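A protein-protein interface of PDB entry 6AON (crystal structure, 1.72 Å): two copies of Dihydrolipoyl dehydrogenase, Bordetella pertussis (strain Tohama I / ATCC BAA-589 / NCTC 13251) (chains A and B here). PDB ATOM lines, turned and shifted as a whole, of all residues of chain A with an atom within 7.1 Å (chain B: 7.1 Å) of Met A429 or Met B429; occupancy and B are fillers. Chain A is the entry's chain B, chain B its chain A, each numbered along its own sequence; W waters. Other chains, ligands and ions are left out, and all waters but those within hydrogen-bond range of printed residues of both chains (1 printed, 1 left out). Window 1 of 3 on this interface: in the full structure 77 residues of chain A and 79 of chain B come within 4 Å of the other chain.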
ATOM      1  N   GLN A  65     -11.653   6.923  17.644  1.00  0.00           N
ATOM      2  CA  GLN A  65     -10.678   8.016  17.545  1.00  0.00           C
ATOM      3  C   GLN A  65     -10.216   8.224  16.110  1.00  0.00           C
ATOM      4  O   GLN A  65     -10.188   9.352  15.613  1.00  0.00           O
ATOM      5  CB  GLN A  65      -9.477   7.784  18.463  1.00  0.00           C
ATOM      6  CG  GLN A  65      -8.567   9.005  18.562  1.00  0.00           C
ATOM      7  CD  GLN A  65      -9.285  10.181  19.164  1.00  0.00           C
ATOM      8  OE1 GLN A  65      -9.842  10.080  20.251  1.00  0.00           O
ATOM      9  NE2 GLN A  65      -9.320  11.297  18.437  1.00  0.00           N
ATOM     10  N   PRO A 367     -20.836  14.312  20.212  1.00  0.00           N
ATOM     11  CA  PRO A 367     -20.148  14.571  21.475  1.00  0.00           C
ATOM     12  C   PRO A 367     -20.105  13.380  22.431  1.00  0.00           C
ATOM     13  O   PRO A 367     -20.916  12.463  22.325  1.00  0.00           O
ATOM     14  CB  PRO A 367     -21.023  15.665  22.117  1.00  0.00           C
ATOM     15  CG  PRO A 367     -22.393  15.421  21.544  1.00  0.00           C
ATOM     16  CD  PRO A 367     -22.152  14.983  20.140  1.00  0.00           C
ATOM     17  N   GLU A 368     -19.154  13.405  23.350  1.00  0.00           N
ATOM     18  CA  GLU A 368     -19.078  12.371  24.391  1.00  0.00           C
ATOM     19  C   GLU A 368     -20.182  12.602  25.401  1.00  0.00           C
ATOM     20  O   GLU A 368     -20.641  13.726  25.601  1.00  0.00           O
ATOM     21  CB  GLU A 368     -17.742  12.395  25.119  1.00  0.00           C
ATOM     22  CG  GLU A 368     -16.583  11.965  24.260  1.00  0.00           C
ATOM     23  CD  GLU A 368     -15.285  11.823  25.029  1.00  0.00           C
ATOM     24  OE1 GLU A 368     -15.276  12.038  26.265  1.00  0.00           O
ATOM     25  OE2 GLU A 368     -14.273  11.490  24.374  1.00  0.00           O
ATOM     26  N   ILE A 369     -20.602  11.518  26.040  1.00  0.00           N
ATOM     27  CA  ILE A 369     -21.640  11.574  27.038  1.00  0.00           C
ATOM     28  C   ILE A 369     -21.147  10.834  28.271  1.00  0.00           C
ATOM     29  O   ILE A 369     -20.586   9.747  28.167  1.00  0.00           O
ATOM     30  CB  ILE A 369     -22.930  10.907  26.509  1.00  0.00           C
ATOM     31  CG1 ILE A 369     -23.468  11.679  25.293  1.00  0.00           C
ATOM     32  CG2 ILE A 369     -23.980  10.845  27.603  1.00  0.00           C
ATOM     33  CD1 ILE A 369     -24.585  10.974  24.554  1.00  0.00           C
ATOM     34  N   ALA A 370     -21.329  11.428  29.441  1.00  0.00           N
ATOM     35  CA  ALA A 370     -20.921  10.758  30.672  1.00  0.00           C
ATOM     36  C   ALA A 370     -21.775  11.176  31.830  1.00  0.00           C
ATOM     37  O   ALA A 370     -22.142  12.339  31.946  1.00  0.00           O
ATOM     38  CB  ALA A 370     -19.467  11.041  30.979  1.00  0.00           C
ATOM     39  N   PHE A 393     -21.551  24.463  27.098  1.00  0.00           N
ATOM     40  CA  PHE A 393     -20.155  24.626  26.676  1.00  0.00           C
ATOM     41  C   PHE A 393     -19.951  25.836  25.793  1.00  0.00           C
ATOM     42  O   PHE A 393     -18.844  26.342  25.719  1.00  0.00           O
ATOM     43  CB  PHE A 393     -19.573  23.353  26.044  1.00  0.00           C
ATOM     44  CG  PHE A 393     -19.257  22.304  27.060  1.00  0.00           C
ATOM     45  CD1 PHE A 393     -18.224  22.508  27.951  1.00  0.00           C
ATOM     46  CD2 PHE A 393     -20.015  21.162  27.169  1.00  0.00           C
ATOM     47  CE1 PHE A 393     -17.940  21.577  28.928  1.00  0.00           C
ATOM     48  CE2 PHE A 393     -19.736  20.218  28.146  1.00  0.00           C
ATOM     49  CZ  PHE A 393     -18.696  20.429  29.022  1.00  0.00           C
ATOM     50  N   ARG A 398     -12.719  27.476  27.343  1.00  0.00           N
ATOM     51  CA  ARG A 398     -11.902  26.421  26.759  1.00  0.00           C
ATOM     52  C   ARG A 398     -12.595  25.775  25.556  1.00  0.00           C
ATOM     53  O   ARG A 398     -11.950  25.476  24.558  1.00  0.00           O
ATOM     54  CB  ARG A 398     -11.581  25.374  27.828  1.00  0.00           C
ATOM     55  CG  ARG A 398     -10.768  24.188  27.368  1.00  0.00           C
ATOM     56  CD  ARG A 398      -9.478  24.605  26.713  1.00  0.00           C
ATOM     57  NE  ARG A 398      -8.624  23.439  26.555  1.00  0.00           N
ATOM     58  CZ  ARG A 398      -7.539  23.375  25.803  1.00  0.00           C
ATOM     59  NH1 ARG A 398      -7.162  24.415  25.045  1.00  0.00           N
ATOM     60  NH2 ARG A 398      -6.838  22.238  25.790  1.00  0.00           N
ATOM     61  N   LEU A 402     -11.194  25.775  21.873  1.00  0.00           N
ATOM     62  CA  LEU A 402     -11.087  24.438  21.272  1.00  0.00           C
ATOM     63  C   LEU A 402     -11.750  24.358  19.900  1.00  0.00           C
ATOM     64  O   LEU A 402     -11.285  23.641  19.007  1.00  0.00           O
ATOM     65  CB  LEU A 402     -11.759  23.413  22.202  1.00  0.00           C
ATOM     66  CG  LEU A 402     -11.494  21.922  22.018  1.00  0.00           C
ATOM     67  CD1 LEU A 402     -10.070  21.619  22.465  1.00  0.00           C
ATOM     68  CD2 LEU A 402     -12.461  21.076  22.838  1.00  0.00           C
ATOM     69  N   ASP A 404     -15.139  23.676  19.779  1.00  0.00           N
ATOM     70  CA  ASP A 404     -16.150  22.640  19.999  1.00  0.00           C
ATOM     71  C   ASP A 404     -16.996  23.067  21.201  1.00  0.00           C
ATOM     72  O   ASP A 404     -16.658  22.791  22.353  1.00  0.00           O
ATOM     73  CB  ASP A 404     -15.473  21.295  20.252  1.00  0.00           C
ATOM     74  CG  ASP A 404     -16.458  20.152  20.398  1.00  0.00           C
ATOM     75  OD1 ASP A 404     -17.694  20.373  20.350  1.00  0.00           O
ATOM     76  OD2 ASP A 404     -15.977  19.022  20.581  1.00  0.00           O
ATOM     77  N   ILE A 425     -23.131  14.928  31.790  1.00  0.00           N
ATOM     78  CA  ILE A 425     -22.366  15.772  30.865  1.00  0.00           C
ATOM     79  C   ILE A 425     -22.418  15.263  29.431  1.00  0.00           C
ATOM     80  O   ILE A 425     -22.212  14.085  29.180  1.00  0.00           O
ATOM     81  CB  ILE A 425     -20.866  15.821  31.266  1.00  0.00           C
ATOM     82  CG1 ILE A 425     -20.686  16.166  32.757  1.00  0.00           C
ATOM     83  CG2 ILE A 425     -20.105  16.827  30.399  1.00  0.00           C
ATOM     84  CD1 ILE A 425     -19.249  16.115  33.235  1.00  0.00           C
ATOM     85  N   GLY A 427     -20.680  16.625  25.841  1.00  0.00           N
ATOM     86  CA  GLY A 427     -19.792  17.599  25.253  1.00  0.00           C
ATOM     87  C   GLY A 427     -18.365  17.119  25.188  1.00  0.00           C
ATOM     88  O   GLY A 427     -18.083  15.935  25.443  1.00  0.00           O
ATOM     89  N   PRO A 428     -17.446  18.035  24.858  1.00  0.00           N
ATOM     90  CA  PRO A 428     -16.068  17.621  24.699  1.00  0.00           C
ATOM     91  C   PRO A 428     -15.462  17.020  25.964  1.00  0.00           C
ATOM     92  O   PRO A 428     -15.653  17.552  27.056  1.00  0.00           O
ATOM     93  CB  PRO A 428     -15.329  18.906  24.286  1.00  0.00           C
ATOM     94  CG  PRO A 428     -16.333  19.996  24.227  1.00  0.00           C
ATOM     95  CD  PRO A 428     -17.687  19.440  24.476  1.00  0.00           C
ATOM     96  N   MET A 429     -14.774  15.890  25.800  1.00  0.00           N
ATOM     97  CA  MET A 429     -14.070  15.203  26.894  1.00  0.00           C
ATOM     98  C   MET A 429     -14.917  14.836  28.105  1.00  0.00           C
ATOM     99  O   MET A 429     -14.387  14.705  29.205  1.00  0.00           O
ATOM    100  CB  MET A 429     -12.883  16.049  27.365  1.00  0.00           C
ATOM    101  CG  MET A 429     -11.782  16.199  26.340  1.00  0.00           C
ATOM    102  SD  MET A 429     -10.939  14.637  26.054  1.00  0.00           S
ATOM    103  CE  MET A 429     -12.134  13.750  25.072  1.00  0.00           C
ATOM    104  N   ALA A 430     -16.220  14.642  27.907  1.00  0.00           N
ATOM    105  CA  ALA A 430     -17.109  14.276  29.010  1.00  0.00           C
ATOM    106  C   ALA A 430     -16.612  13.055  29.794  1.00  0.00           C
ATOM    107  O   ALA A 430     -16.759  13.006  31.010  1.00  0.00           O
ATOM    108  CB  ALA A 430     -18.508  14.018  28.510  1.00  0.00           C
ATOM    109  N   SER A 431     -16.033  12.091  29.074  1.00  0.00           N
ATOM    110  CA  SER A 431     -15.485  10.863  29.668  1.00  0.00           C
ATOM    111  C   SER A 431     -14.459  11.152  30.776  1.00  0.00           C
ATOM    112  O   SER A 431     -14.374  10.411  31.764  1.00  0.00           O
ATOM    113  CB  SER A 431     -14.830  10.012  28.583  1.00  0.00           C
ATOM    114  OG  SER A 431     -13.788  10.713  27.919  1.00  0.00           O
ATOM    115  N   GLU A 432     -13.696  12.227  30.610  1.00  0.00           N
ATOM    116  CA  GLU A 432     -12.673  12.606  31.587  1.00  0.00           C
ATOM    117  C   GLU A 432     -13.237  13.543  32.644  1.00  0.00           C
ATOM    118  O   GLU A 432     -12.911  13.410  33.832  1.00  0.00           O
ATOM    119  CB  GLU A 432     -11.468  13.245  30.893  1.00  0.00           C
ATOM    120  CG  GLU A 432     -10.829  12.374  29.813  1.00  0.00           C
ATOM    121  CD  GLU A 432     -10.281  11.048  30.335  1.00  0.00           C
ATOM    122  OE1 GLU A 432     -10.133  10.883  31.573  1.00  0.00           O
ATOM    123  OE2 GLU A 432      -9.964  10.172  29.488  1.00  0.00           O
ATOM    124  N   LEU A 433     -14.117  14.453  32.234  1.00  0.00           N
ATOM    125  CA  LEU A 433     -14.715  15.406  33.173  1.00  0.00           C
ATOM    126  C   LEU A 433     -15.532  14.733  34.263  1.00  0.00           C
ATOM    127  O   LEU A 433     -15.639  15.262  35.366  1.00  0.00           O
ATOM    128  CB  LEU A 433     -15.613  16.416  32.445  1.00  0.00           C
ATOM    129  CG  LEU A 433     -14.969  17.237  31.324  1.00  0.00           C
ATOM    130  CD1 LEU A 433     -15.952  18.285  30.842  1.00  0.00           C
ATOM    131  CD2 LEU A 433     -13.667  17.880  31.763  1.00  0.00           C
ATOM    132  N   ILE A 434     -16.085  13.554  33.981  1.00  0.00           N
ATOM    133  CA  ILE A 434     -16.963  12.910  34.956  1.00  0.00           C
ATOM    134  C   ILE A 434     -16.244  12.427  36.223  1.00  0.00           C
ATOM    135  O   ILE A 434     -16.881  12.269  37.264  1.00  0.00           O
ATOM    136  CB  ILE A 434     -17.773  11.757  34.323  1.00  0.00           C
ATOM    137  CG1 ILE A 434     -19.065  11.486  35.119  1.00  0.00           C
ATOM    138  CG2 ILE A 434     -16.923  10.521  34.129  1.00  0.00           C
ATOM    139  CD1 ILE A 434     -20.016  12.668  35.136  1.00  0.00           C
ATOM    140  N   LEU A 460     -12.477  22.875  30.346  1.00  0.00           N
ATOM    141  CA  LEU A 460     -13.836  22.332  30.198  1.00  0.00           C
ATOM    142  C   LEU A 460     -14.433  21.999  31.574  1.00  0.00           C
ATOM    143  O   LEU A 460     -15.653  22.130  31.789  1.00  0.00           O
ATOM    144  CB  LEU A 460     -13.807  21.084  29.308  1.00  0.00           C
ATOM    145  CG  LEU A 460     -13.349  21.291  27.862  1.00  0.00           C
ATOM    146  CD1 LEU A 460     -13.059  19.956  27.216  1.00  0.00           C
ATOM    147  CD2 LEU A 460     -14.362  22.081  27.042  1.00  0.00           C
ATOM    148  N   PRO B 367       2.967  17.486  25.082  1.00  0.00           N
ATOM    149  CA  PRO B 367       1.906  17.138  26.029  1.00  0.00           C
ATOM    150  C   PRO B 367       1.556  18.275  26.972  1.00  0.00           C
ATOM    151  O   PRO B 367       2.353  19.203  27.155  1.00  0.00           O
ATOM    152  CB  PRO B 367       2.528  16.005  26.842  1.00  0.00           C
ATOM    153  CG  PRO B 367       3.989  16.308  26.842  1.00  0.00           C
ATOM    154  CD  PRO B 367       4.278  16.958  25.511  1.00  0.00           C
ATOM    155  N   GLU B 368       0.353  18.211  27.548  1.00  0.00           N
ATOM    156  CA  GLU B 368      -0.065  19.204  28.508  1.00  0.00           C
ATOM    157  C   GLU B 368       0.607  18.865  29.821  1.00  0.00           C
ATOM    158  O   GLU B 368       1.050  17.728  30.028  1.00  0.00           O
ATOM    159  CB  GLU B 368      -1.587  19.217  28.697  1.00  0.00           C
ATOM    160  CG  GLU B 368      -2.358  19.562  27.434  1.00  0.00           C
ATOM    161  CD  GLU B 368      -3.849  19.756  27.669  1.00  0.00           C
ATOM    162  OE1 GLU B 368      -4.348  19.485  28.779  1.00  0.00           O
ATOM    163  OE2 GLU B 368      -4.526  20.184  26.721  1.00  0.00           O
ATOM    164  N   ILE B 369       0.697  19.862  30.685  1.00  0.00           N
ATOM    165  CA  ILE B 369       1.296  19.722  31.999  1.00  0.00           C
ATOM    166  C   ILE B 369       0.363  20.417  32.951  1.00  0.00           C
ATOM    167  O   ILE B 369      -0.042  21.536  32.688  1.00  0.00           O
ATOM    168  CB  ILE B 369       2.691  20.388  32.083  1.00  0.00           C
ATOM    169  CG1 ILE B 369       3.630  19.777  31.029  1.00  0.00           C
ATOM    170  CG2 ILE B 369       3.296  20.209  33.478  1.00  0.00           C
ATOM    171  CD1 ILE B 369       4.905  20.558  30.819  1.00  0.00           C
ATOM    172  N   ALA B 370       0.021  19.744  34.040  1.00  0.00           N
ATOM    173  CA  ALA B 370      -0.854  20.307  35.050  1.00  0.00           C
ATOM    174  C   ALA B 370      -0.472  19.755  36.415  1.00  0.00           C
ATOM    175  O   ALA B 370      -0.136  18.571  36.548  1.00  0.00           O
ATOM    176  CB  ALA B 370      -2.307  19.986  34.733  1.00  0.00           C
ATOM    177  N   PHE B 393       1.330   6.876  31.024  1.00  0.00           N
ATOM    178  CA  PHE B 393       0.223   6.771  30.065  1.00  0.00           C
ATOM    179  C   PHE B 393       0.433   5.631  29.049  1.00  0.00           C
ATOM    180  O   PHE B 393      -0.527   5.157  28.439  1.00  0.00           O
ATOM    181  CB  PHE B 393      -0.086   8.123  29.386  1.00  0.00           C
ATOM    182  CG  PHE B 393      -0.756   9.102  30.304  1.00  0.00           C
ATOM    183  CD1 PHE B 393      -2.097   8.926  30.656  1.00  0.00           C
ATOM    184  CD2 PHE B 393      -0.063  10.178  30.844  1.00  0.00           C
ATOM    185  CE1 PHE B 393      -2.720   9.808  31.524  1.00  0.00           C
ATOM    186  CE2 PHE B 393      -0.687  11.070  31.705  1.00  0.00           C
ATOM    187  CZ  PHE B 393      -2.015  10.893  32.038  1.00  0.00           C
ATOM    188  N   ARG B 398      -6.842   4.155  27.495  1.00  0.00           N
ATOM    189  CA  ARG B 398      -7.410   5.276  26.747  1.00  0.00           C
ATOM    190  C   ARG B 398      -6.326   5.956  25.933  1.00  0.00           C
ATOM    191  O   ARG B 398      -6.537   6.253  24.751  1.00  0.00           O
ATOM    192  CB  ARG B 398      -8.098   6.295  27.659  1.00  0.00           C
ATOM    193  CG  ARG B 398      -8.725   7.473  26.903  1.00  0.00           C
ATOM    194  CD  ARG B 398      -9.911   7.038  26.067  1.00  0.00           C
ATOM    195  NE  ARG B 398     -10.417   8.059  25.144  1.00  0.00           N
ATOM    196  CZ  ARG B 398     -11.132   9.139  25.480  1.00  0.00           C
ATOM    197  NH1 ARG B 398     -11.390   9.456  26.761  1.00  0.00           N
ATOM    198  NH2 ARG B 398     -11.558   9.955  24.512  1.00  0.00           N
ATOM    199  N   LEU B 402      -6.279   6.331  21.967  1.00  0.00           N
ATOM    200  CA  LEU B 402      -6.135   7.688  21.439  1.00  0.00           C
ATOM    201  C   LEU B 402      -4.986   7.813  20.445  1.00  0.00           C
ATOM    202  O   LEU B 402      -5.092   8.552  19.452  1.00  0.00           O
ATOM    203  CB  LEU B 402      -5.899   8.671  22.594  1.00  0.00           C
ATOM    204  CG  LEU B 402      -5.641  10.150  22.289  1.00  0.00           C
ATOM    205  CD1 LEU B 402      -6.850  10.795  21.636  1.00  0.00           C
ATOM    206  CD2 LEU B 402      -5.277  10.902  23.558  1.00  0.00           C
ATOM    207  N   ASP B 404      -1.809   8.550  21.697  1.00  0.00           N
ATOM    208  CA  ASP B 404      -0.944   9.537  22.340  1.00  0.00           C
ATOM    209  C   ASP B 404      -0.654   8.992  23.744  1.00  0.00           C
ATOM    210  O   ASP B 404      -1.443   9.202  24.680  1.00  0.00           O
ATOM    211  CB  ASP B 404      -1.622  10.907  22.403  1.00  0.00           C
ATOM    212  CG  ASP B 404      -0.750  11.975  23.067  1.00  0.00           C
ATOM    213  OD1 ASP B 404       0.429  11.695  23.412  1.00  0.00           O
ATOM    214  OD2 ASP B 404      -1.262  13.104  23.241  1.00  0.00           O
ATOM    215  N   ILE B 425       0.902  15.954  36.725  1.00  0.00           N
ATOM    216  CA  ILE B 425       0.565  15.211  35.522  1.00  0.00           C
ATOM    217  C   ILE B 425       1.167  15.836  34.265  1.00  0.00           C
ATOM    218  O   ILE B 425       1.097  17.049  34.066  1.00  0.00           O
ATOM    219  CB  ILE B 425      -0.980  15.151  35.335  1.00  0.00           C
ATOM    220  CG1 ILE B 425      -1.690  14.749  36.653  1.00  0.00           C
ATOM    221  CG2 ILE B 425      -1.352  14.218  34.182  1.00  0.00           C
ATOM    222  CD1 ILE B 425      -3.194  14.726  36.587  1.00  0.00           C
ATOM    223  N   GLY B 427       0.943  14.799  30.188  1.00  0.00           N
ATOM    224  CA  GLY B 427       0.315  13.879  29.253  1.00  0.00           C
ATOM    225  C   GLY B 427      -0.926  14.459  28.615  1.00  0.00           C
ATOM    226  O   GLY B 427      -1.247  15.661  28.806  1.00  0.00           O
ATOM    227  N   PRO B 428      -1.653  13.614  27.870  1.00  0.00           N
ATOM    228  CA  PRO B 428      -2.848  14.097  27.193  1.00  0.00           C
ATOM    229  C   PRO B 428      -3.934  14.584  28.154  1.00  0.00           C
ATOM    230  O   PRO B 428      -4.177  13.957  29.172  1.00  0.00           O
ATOM    231  CB  PRO B 428      -3.325  12.891  26.346  1.00  0.00           C
ATOM    232  CG  PRO B 428      -2.447  11.740  26.686  1.00  0.00           C
ATOM    233  CD  PRO B 428      -1.339  12.198  27.579  1.00  0.00           C
ATOM    234  N   MET B 429      -4.537  15.729  27.836  1.00  0.00           N
ATOM    235  CA  MET B 429      -5.640  16.305  28.630  1.00  0.00           C
ATOM    236  C   MET B 429      -5.331  16.556  30.103  1.00  0.00           C
ATOM    237  O   MET B 429      -6.247  16.653  30.916  1.00  0.00           O
ATOM    238  CB  MET B 429      -6.863  15.386  28.555  1.00  0.00           C
ATOM    239  CG  MET B 429      -7.322  15.091  27.142  1.00  0.00           C
ATOM    240  SD  MET B 429      -7.674  16.620  26.271  1.00  0.00           S
ATOM    241  CE  MET B 429      -8.750  17.431  27.439  1.00  0.00           C
ATOM    242  N   ALA B 430      -4.054  16.672  30.449  1.00  0.00           N
ATOM    243  CA  ALA B 430      -3.656  16.904  31.858  1.00  0.00           C
ATOM    244  C   ALA B 430      -4.390  18.096  32.496  1.00  0.00           C
ATOM    245  O   ALA B 430      -4.722  18.061  33.683  1.00  0.00           O
ATOM    246  CB  ALA B 430      -2.147  17.094  31.963  1.00  0.00           C
ATOM    247  N   SER B 431      -4.655  19.121  31.688  1.00  0.00           N
ATOM    248  CA  SER B 431      -5.377  20.311  32.142  1.00  0.00           C
ATOM    249  C   SER B 431      -6.756  19.982  32.729  1.00  0.00           C
ATOM    250  O   SER B 431      -7.235  20.690  33.628  1.00  0.00           O
ATOM    251  CB  SER B 431      -5.570  21.286  30.985  1.00  0.00           C
ATOM    252  OG  SER B 431      -6.355  20.716  29.940  1.00  0.00           O
ATOM    253  N   GLU B 432      -7.394  18.936  32.187  1.00  0.00           N
ATOM    254  CA  GLU B 432      -8.712  18.512  32.640  1.00  0.00           C
ATOM    255  C   GLU B 432      -8.578  17.481  33.745  1.00  0.00           C
ATOM    256  O   GLU B 432      -9.320  17.535  34.704  1.00  0.00           O
ATOM    257  CB  GLU B 432      -9.570  17.949  31.486  1.00  0.00           C
ATOM    258  CG  GLU B 432      -9.769  18.881  30.296  1.00  0.00           C
ATOM    259  CD  GLU B 432     -10.474  20.190  30.616  1.00  0.00           C
ATOM    260  OE1 GLU B 432     -11.104  20.320  31.692  1.00  0.00           O
ATOM    261  OE2 GLU B 432     -10.406  21.108  29.770  1.00  0.00           O
ATOM    262  N   LEU B 433      -7.604  16.584  33.644  1.00  0.00           N
ATOM    263  CA  LEU B 433      -7.436  15.557  34.672  1.00  0.00           C
ATOM    264  C   LEU B 433      -7.106  16.130  36.056  1.00  0.00           C
ATOM    265  O   LEU B 433      -7.445  15.535  37.068  1.00  0.00           O
ATOM    266  CB  LEU B 433      -6.331  14.594  34.291  1.00  0.00           C
ATOM    267  CG  LEU B 433      -6.425  13.947  32.918  1.00  0.00           C
ATOM    268  CD1 LEU B 433      -5.233  13.031  32.746  1.00  0.00           C
ATOM    269  CD2 LEU B 433      -7.749  13.226  32.711  1.00  0.00           C
ATOM    270  N   ILE B 434      -6.454  17.287  36.097  1.00  0.00           N
ATOM    271  CA  ILE B 434      -6.039  17.872  37.377  1.00  0.00           C
ATOM    272  C   ILE B 434      -7.224  18.298  38.261  1.00  0.00           C
ATOM    273  O   ILE B 434      -7.076  18.370  39.477  1.00  0.00           O
ATOM    274  CB  ILE B 434      -5.053  19.050  37.162  1.00  0.00           C
ATOM    275  CG1 ILE B 434      -4.155  19.281  38.395  1.00  0.00           C
ATOM    276  CG2 ILE B 434      -5.796  20.324  36.744  1.00  0.00           C
ATOM    277  CD1 ILE B 434      -3.263  18.104  38.730  1.00  0.00           C
ATOM    278  N   LEU B 460      -8.277   8.390  30.598  1.00  0.00           N
ATOM    279  CA  LEU B 460      -6.978   8.886  31.045  1.00  0.00           C
ATOM    280  C   LEU B 460      -6.970   9.086  32.557  1.00  0.00           C
ATOM    281  O   LEU B 460      -5.927   8.912  33.202  1.00  0.00           O
ATOM    282  CB  LEU B 460      -6.642  10.199  30.345  1.00  0.00           C
ATOM    283  CG  LEU B 460      -6.541  10.126  28.836  1.00  0.00           C
ATOM    284  CD1 LEU B 460      -6.582  11.529  28.273  1.00  0.00           C
ATOM    285  CD2 LEU B 460      -5.294   9.371  28.384  1.00  0.00           C
HETATM  286  O   HOH W   1      -8.230  21.800  28.376  1.00  0.00           O
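Glu A368 touches Arg B398, and with the chains exchanged Arg A398 touches Glu B368.
Arg A398 touches Glu B432, and with the chains exchanged Glu A432 touches Arg B398.
Met B429 touches its own counterpart, Met A429.
Ser A431 touches Arg B398, but with the chains exchanged Arg A398 does not touch Ser B431 (4.4 Å).
Of the 12 pairs that touch across the chains among the printed residues, 9 have their exchanged pair printed and touching as well.
The backbone NH (N) of Ala B430 is in hydrogen-bond range of the side-chain carboxylate (OE1) of Glu B368, 3.3 Å away.
O of Glu A368 is in hydrogen-bond range of N of Gly A427 (2.9 Å).
The backbone NH (N) of Ala A430 sits at hydrogen-bond distance from the side-chain carboxylate (OE1) of Glu A368.
The side-chain carboxylate of Glu B368 lies within hydrogen-bond range of the side-chain hydroxyl of Ser B431, 2.6 Å away.
The backbone NH (N) of Gly B427 is in hydrogen-bond range of the backbone carbonyl oxygen (O) of Glu B368 (2.9 Å).
OE1 of Glu A368 is in hydrogen-bond range of OG of Ser A431 (2.6 Å).
Gln A65 touches Leu B402.
CG of Arg A398 touches OE2 of Glu B432 (3.9 Å).
Met A429 touches Arg B398 (CE to NH2, 3.9 Å).
Met A429 touches Met B429.
Glu A432 touches Leu B433.
Leu A433 touches Glu B432.
Of the 19 printed residues of chain A, 8 touch a printed residue of chain B.
Hydrophobic or aromatic side chains of chain A within 4 Å of the printed part of chain B: Met A429, Leu A433 and Leu A460.
Hydrophobic or aromatic side chains of chain B that line the printed part of chain A: Leu B402, Met B429, Leu B433 and Leu B460.
Along chain B the printed residues that touch a printed residue of chain A span positions 368 to 460.
Among the printed residues, 12 pairs touch across the chains.
The guanidinium group of Arg B398 lies within hydrogen-bond range of the side-chain hydroxyl of Ser A431 (2.9 Å).
The side-chain carboxylate of Glu B432 lies within hydrogen-bond range of the backbone NH of Leu A460 (2.8 Å).
The side-chain carboxylate of Glu A368 is in salt-bridge range of the guanidinium group of Arg B398 (3.1 Å).
The guanidinium group (NH1) of Arg B398 is in salt-bridge range of the side-chain carboxylate (OE2) of Glu A432, at 3.2 Å.
OE2 of Glu A432 sits at hydrogen-bond distance from N of Leu B460, 2.7 Å away.
OE2 of Glu B368 lies within salt-bridge range of NH2 of Arg A398, 3.2 Å away.
Ile A425 touches none of the printed residues of chain B.
Of the printed residues of chain B, Met A429 touches Arg B398 and Met B429.
Of the printed residues of chain B, Glu A432 touches Arg B398, Leu B433 and Leu B460.
Printed residues of chain A within 4 Å of Leu B402: Gln A65.
The nearest printed residue of chain B that does not touch Met A429 is Glu B432 (5.1 Å).
Water W1 lies within hydrogen-bond range of NE of Arg A398 (2.5 Å), OG of Ser B431 (2.7 Å) and OE2 of Glu B432 (2.7 Å).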
